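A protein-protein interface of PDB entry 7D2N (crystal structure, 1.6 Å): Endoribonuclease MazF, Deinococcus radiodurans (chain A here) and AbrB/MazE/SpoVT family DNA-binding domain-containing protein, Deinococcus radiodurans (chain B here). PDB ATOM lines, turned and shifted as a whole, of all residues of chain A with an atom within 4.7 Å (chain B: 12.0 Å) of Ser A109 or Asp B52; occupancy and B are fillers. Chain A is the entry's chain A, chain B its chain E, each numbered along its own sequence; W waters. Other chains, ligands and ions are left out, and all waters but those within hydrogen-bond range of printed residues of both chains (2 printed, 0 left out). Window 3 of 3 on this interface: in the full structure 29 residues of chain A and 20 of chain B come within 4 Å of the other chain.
The side-chain carboxylate (OD2) of Asp B52 sits at hydrogen-bond distance from the backbone NH (N) of Ala B54, 3.0 Å away. The backbone NH (N) of Ala B55 lies within hydrogen-bond range of the side-chain carboxylate (OD2) of Asp B52 (2.6 Å).
Of chain B, only Tyr B51 (2.7 Å), Asp B52 (3.7 Å) and Leu B53 (3.1 Å) come within 4 Å of Ser A109. Asp B52 touches one residue of chain A. No residue of chain B comes within 4 Å of Leu A107. Gly A108 touches none of the printed residues of chain B. Leu A110 touches one residue of chain B. No residue of chain B comes within 4 Å of Leu A111. No residue of chain B comes within 4 Å of Gly A112. Printed residues of chain A within 4 Å of Tyr B51: Gly A105 (3.5 Å), Lys A106 (3.8 Å) and Ser A109 (2.7 Å). Of the printed residues of chain A, Leu B53 touches Ser A109 (3.1 Å) and Leu A110 (3.9 Å). Arg A104 touches none of the printed residues of chain B. Ala B55 touches none of the printed residues of chain A. The nearest residue of chain B that does not touch Ser A109 is Leu B56 (4.4 Å). The nearest printed residue of chain A that does not touch Asp B52 is Gly A105 (6.5 Å). The nearest printed residue of chain B that does not touch Lys A106 is Leu B56 (4.1 Å).
OG of Ser A109 lies within hydrogen-bond range of N of Leu B53 (3.1 Å). The side-chain hydroxyl (OG) of Ser A109 sits at hydrogen-bond distance from the backbone carbonyl oxygen (O) of Tyr B51 (2.7 Å).
Printed residues of chain B that touch a printed residue of chain A: Tyr B51, Asp B52 and Leu B53. Hydrophobic or aromatic side chains of chain B that line the printed part of chain A: Tyr B51 and Leu B53. Of the 9 printed residues of chain A, 4 touch a printed residue of chain B. Among the printed residues, no Asp or Glu carboxylate lies within 4 Å of a Lys or Arg side-chain nitrogen of the other chain.
Among the printed residues, merely in contact across the chains: Gly A105 with Tyr B51 (3.5 Å), Lys A106 with Tyr B51 (3.8 Å), Ser A109 with Asp B52 (3.7 Å) and Leu A110 with Leu B53 (3.9 Å).
Water W1 bridges N of Leu B53 and OG of Ser A109. Water W2 lies within hydrogen-bond range of O of Gly A105 (2.8 Å) and N of Tyr B51 (3.5 Å).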
ATOM      1  N   ARG A 104      38.912   4.305  -9.843  1.00  0.00           N
ATOM      2  CA  ARG A 104      38.857   5.652 -10.400  1.00  0.00           C
ATOM      3  C   ARG A 104      37.828   5.748 -11.516  1.00  0.00           C
ATOM      4  O   ARG A 104      37.136   6.761 -11.642  1.00  0.00           O
ATOM      5  CB  ARG A 104      40.232   6.065 -10.916  1.00  0.00           C
ATOM      6  CG  ARG A 104      41.208   6.413  -9.812  1.00  0.00           C
ATOM      7  CD  ARG A 104      42.626   6.524 -10.343  1.00  0.00           C
ATOM      8  NE  ARG A 104      43.503   7.153  -9.359  1.00  0.00           N
ATOM      9  CZ  ARG A 104      44.824   7.061  -9.368  1.00  0.00           C
ATOM     10  NH1 ARG A 104      45.442   6.370 -10.327  1.00  0.00           N
ATOM     11  NH2 ARG A 104      45.532   7.673  -8.424  1.00  0.00           N
ATOM     12  N   GLY A 105      37.716   4.711 -12.345  1.00  0.00           N
ATOM     13  CA  GLY A 105      36.727   4.750 -13.405  1.00  0.00           C
ATOM     14  C   GLY A 105      35.307   4.798 -12.877  1.00  0.00           C
ATOM     15  O   GLY A 105      34.475   5.570 -13.361  1.00  0.00           O
ATOM     16  N   LYS A 106      35.007   3.974 -11.874  1.00  0.00           N
ATOM     17  CA  LYS A 106      33.657   3.976 -11.318  1.00  0.00           C
ATOM     18  C   LYS A 106      33.368   5.269 -10.567  1.00  0.00           C
ATOM     19  O   LYS A 106      32.293   5.858 -10.722  1.00  0.00           O
ATOM     20  CB  LYS A 106      33.457   2.767 -10.409  1.00  0.00           C
ATOM     21  CG  LYS A 106      33.365   1.456 -11.186  1.00  0.00           C
ATOM     22  CD  LYS A 106      33.338   0.264 -10.259  1.00  0.00           C
ATOM     23  CE  LYS A 106      33.113  -1.028 -11.050  1.00  0.00           C
ATOM     24  NZ  LYS A 106      32.946  -2.213 -10.149  1.00  0.00           N
ATOM     25  N   LEU A 107      34.319   5.733  -9.756  1.00  0.00           N
ATOM     26  CA  LEU A 107      34.109   6.982  -9.034  1.00  0.00           C
ATOM     27  C   LEU A 107      34.016   8.162  -9.993  1.00  0.00           C
ATOM     28  O   LEU A 107      33.158   9.035  -9.826  1.00  0.00           O
ATOM     29  CB  LEU A 107      35.232   7.198  -8.014  1.00  0.00           C
ATOM     30  CG  LEU A 107      35.213   8.523  -7.254  1.00  0.00           C
ATOM     31  CD1 LEU A 107      33.943   8.647  -6.439  1.00  0.00           C
ATOM     32  CD2 LEU A 107      36.457   8.625  -6.349  1.00  0.00           C
ATOM     33  N   GLY A 108      34.899   8.216 -10.995  1.00  0.00           N
ATOM     34  CA  GLY A 108      34.849   9.316 -11.948  1.00  0.00           C
ATOM     35  C   GLY A 108      33.527   9.379 -12.685  1.00  0.00           C
ATOM     36  O   GLY A 108      32.990  10.464 -12.919  1.00  0.00           O
ATOM     37  N   SER A 109      32.976   8.215 -13.037  1.00  0.00           N
ATOM     38  CA  SER A 109      31.648   8.164 -13.644  1.00  0.00           C
ATOM     39  C   SER A 109      30.602   8.800 -12.733  1.00  0.00           C
ATOM     40  O   SER A 109      29.797   9.637 -13.170  1.00  0.00           O
ATOM     41  CB  SER A 109      31.286   6.708 -13.958  1.00  0.00           C
ATOM     42  OG  SER A 109      30.090   6.629 -14.707  1.00  0.00           O
ATOM     43  N   LEU A 110      30.618   8.429 -11.448  1.00  0.00           N
ATOM     44  CA  LEU A 110      29.653   8.965 -10.495  1.00  0.00           C
ATOM     45  C   LEU A 110      29.798  10.475 -10.340  1.00  0.00           C
ATOM     46  O   LEU A 110      28.793  11.192 -10.223  1.00  0.00           O
ATOM     47  CB  LEU A 110      29.833   8.268  -9.148  1.00  0.00           C
ATOM     48  CG  LEU A 110      28.947   8.793  -8.028  1.00  0.00           C
ATOM     49  CD1 LEU A 110      27.484   8.591  -8.404  1.00  0.00           C
ATOM     50  CD2 LEU A 110      29.280   8.075  -6.733  1.00  0.00           C
ATOM     51  N   LEU A 111      31.036  10.977 -10.335  1.00  0.00           N
ATOM     52  CA  LEU A 111      31.275  12.402 -10.131  1.00  0.00           C
ATOM     53  C   LEU A 111      30.969  13.241 -11.361  1.00  0.00           C
ATOM     54  O   LEU A 111      31.018  14.474 -11.276  1.00  0.00           O
ATOM     55  CB  LEU A 111      32.732  12.644  -9.710  1.00  0.00           C
ATOM     56  CG  LEU A 111      33.088  12.031  -8.356  1.00  0.00           C
ATOM     57  CD1 LEU A 111      34.567  12.168  -8.076  1.00  0.00           C
ATOM     58  CD2 LEU A 111      32.280  12.701  -7.252  1.00  0.00           C
ATOM     59  N   GLY A 112      30.660  12.611 -12.490  1.00  0.00           N
ATOM     60  CA  GLY A 112      30.427  13.357 -13.708  1.00  0.00           C
ATOM     61  C   GLY A 112      31.675  13.860 -14.389  1.00  0.00           C
ATOM     62  O   GLY A 112      31.626  14.903 -15.053  1.00  0.00           O
ATOM     63  N   TYR B  51      33.611   3.900 -17.829  1.00  0.00           N
ATOM     64  CA  TYR B  51      32.484   3.311 -17.110  1.00  0.00           C
ATOM     65  C   TYR B  51      31.230   4.164 -17.281  1.00  0.00           C
ATOM     66  O   TYR B  51      31.190   5.325 -16.862  1.00  0.00           O
ATOM     67  CB  TYR B  51      32.808   3.150 -15.619  1.00  0.00           C
ATOM     68  CG  TYR B  51      33.813   2.065 -15.327  1.00  0.00           C
ATOM     69  CD1 TYR B  51      35.176   2.311 -15.434  1.00  0.00           C
ATOM     70  CD2 TYR B  51      33.404   0.788 -14.960  1.00  0.00           C
ATOM     71  CE1 TYR B  51      36.102   1.316 -15.177  1.00  0.00           C
ATOM     72  CE2 TYR B  51      34.324  -0.217 -14.699  1.00  0.00           C
ATOM     73  CZ  TYR B  51      35.673   0.055 -14.808  1.00  0.00           C
ATOM     74  OH  TYR B  51      36.600  -0.932 -14.554  1.00  0.00           O
ATOM     75  N   ASP B  52      30.205   3.585 -17.903  1.00  0.00           N
ATOM     76  CA  ASP B  52      28.946   4.290 -18.113  1.00  0.00           C
ATOM     77  C   ASP B  52      28.163   4.306 -16.809  1.00  0.00           C
ATOM     78  O   ASP B  52      27.889   3.245 -16.237  1.00  0.00           O
ATOM     79  CB  ASP B  52      28.136   3.609 -19.215  1.00  0.00           C
ATOM     80  CG  ASP B  52      26.743   4.190 -19.360  1.00  0.00           C
ATOM     81  OD1 ASP B  52      26.599   5.215 -20.059  1.00  0.00           O
ATOM     82  OD2 ASP B  52      25.790   3.626 -18.777  1.00  0.00           O
ATOM     83  N   LEU B  53      27.777   5.503 -16.349  1.00  0.00           N
ATOM     84  CA  LEU B  53      27.087   5.601 -15.066  1.00  0.00           C
ATOM     85  C   LEU B  53      25.747   4.872 -15.092  1.00  0.00           C
ATOM     86  O   LEU B  53      25.394   4.182 -14.131  1.00  0.00           O
ATOM     87  CB  LEU B  53      26.894   7.062 -14.673  1.00  0.00           C
ATOM     88  CG  LEU B  53      26.326   7.268 -13.265  1.00  0.00           C
ATOM     89  CD1 LEU B  53      27.150   6.533 -12.198  1.00  0.00           C
ATOM     90  CD2 LEU B  53      26.212   8.760 -12.925  1.00  0.00           C
ATOM     91  N   ALA B  54      24.985   5.006 -16.182  1.00  0.00           N
ATOM     92  CA  ALA B  54      23.682   4.350 -16.226  1.00  0.00           C
ATOM     93  C   ALA B  54      23.823   2.838 -16.098  1.00  0.00           C
ATOM     94  O   ALA B  54      23.013   2.187 -15.427  1.00  0.00           O
ATOM     95  CB  ALA B  54      22.944   4.717 -17.512  1.00  0.00           C
ATOM     96  N   ALA B  55      24.852   2.266 -16.730  1.00  0.00           N
ATOM     97  CA  ALA B  55      25.084   0.829 -16.606  1.00  0.00           C
ATOM     98  C   ALA B  55      25.380   0.446 -15.161  1.00  0.00           C
ATOM     99  O   ALA B  55      24.882  -0.570 -14.663  1.00  0.00           O
ATOM    100  CB  ALA B  55      26.231   0.401 -17.523  1.00  0.00           C
ATOM    101  N   LEU B  56      26.164   1.265 -14.459  1.00  0.00           N
ATOM    102  CA  LEU B  56      26.410   0.997 -13.049  1.00  0.00           C
ATOM    103  C   LEU B  56      25.126   1.095 -12.234  1.00  0.00           C
ATOM    104  O   LEU B  56      24.802   0.188 -11.464  1.00  0.00           O
ATOM    105  CB  LEU B  56      27.464   1.963 -12.505  1.00  0.00           C
ATOM    106  CG  LEU B  56      28.883   1.754 -13.020  1.00  0.00           C
ATOM    107  CD1 LEU B  56      29.772   2.868 -12.508  1.00  0.00           C
ATOM    108  CD2 LEU B  56      29.412   0.393 -12.585  1.00  0.00           C
ATOM    109  N   LEU B  57      24.384   2.201 -12.380  1.00  0.00           N
ATOM    110  CA  LEU B  57      23.197   2.402 -11.553  1.00  0.00           C
ATOM    111  C   LEU B  57      22.140   1.342 -11.827  1.00  0.00           C
ATOM    112  O   LEU B  57      21.375   0.993 -10.923  1.00  0.00           O
ATOM    113  CB  LEU B  57      22.612   3.797 -11.774  1.00  0.00           C
ATOM    114  CG  LEU B  57      23.541   4.991 -11.563  1.00  0.00           C
ATOM    115  CD1 LEU B  57      22.817   6.304 -11.835  1.00  0.00           C
ATOM    116  CD2 LEU B  57      24.133   4.964 -10.147  1.00  0.00           C
ATOM    117  N   ALA B  58      22.102   0.799 -13.052  1.00  0.00           N
ATOM    118  CA  ALA B  58      21.151  -0.262 -13.374  1.00  0.00           C
ATOM    119  C   ALA B  58      21.399  -1.534 -12.575  1.00  0.00           C
ATOM    120  O   ALA B  58      20.503  -2.380 -12.492  1.00  0.00           O
ATOM    121  CB  ALA B  58      21.193  -0.583 -14.870  1.00  0.00           C
ATOM    122  N   GLU B  59      22.585  -1.694 -11.985  1.00  0.00           N
ATOM    123  CA  GLU B  59      22.904  -2.896 -11.225  1.00  0.00           C
ATOM    124  C   GLU B  59      22.645  -2.738  -9.733  1.00  0.00           C
ATOM    125  O   GLU B  59      22.856  -3.692  -8.978  1.00  0.00           O
ATOM    126  CB  GLU B  59      24.367  -3.300 -11.453  1.00  0.00           C
ATOM    127  CG  GLU B  59      24.652  -3.871 -12.841  1.00  0.00           C
ATOM    128  CD  GLU B  59      23.793  -5.095 -13.176  1.00  0.00           C
ATOM    129  OE1 GLU B  59      22.869  -4.960 -14.011  1.00  0.00           O
ATOM    130  OE2 GLU B  59      24.046  -6.192 -12.616  1.00  0.00           O
ATOM    131  N   MET B  60      22.205  -1.568  -9.287  1.00  0.00           N
ATOM    132  CA  MET B  60      21.893  -1.379  -7.880  1.00  0.00           C
ATOM    133  C   MET B  60      20.539  -1.984  -7.543  1.00  0.00           C
ATOM    134  O   MET B  60      19.625  -1.996  -8.370  1.00  0.00           O
ATOM    135  CB  MET B  60      21.908   0.099  -7.515  1.00  0.00           C
ATOM    136  CG  MET B  60      23.266   0.739  -7.728  1.00  0.00           C
ATOM    137  SD  MET B  60      23.274   2.467  -7.252  1.00  0.00           S
ATOM    138  CE  MET B  60      22.590   2.257  -5.675  1.00  0.00           C
HETATM  139  O   HOH W   1      28.674   7.799 -17.447  1.00  0.00           O
HETATM  140  O   HOH W   2      34.721   6.617 -15.971  1.00  0.00           O
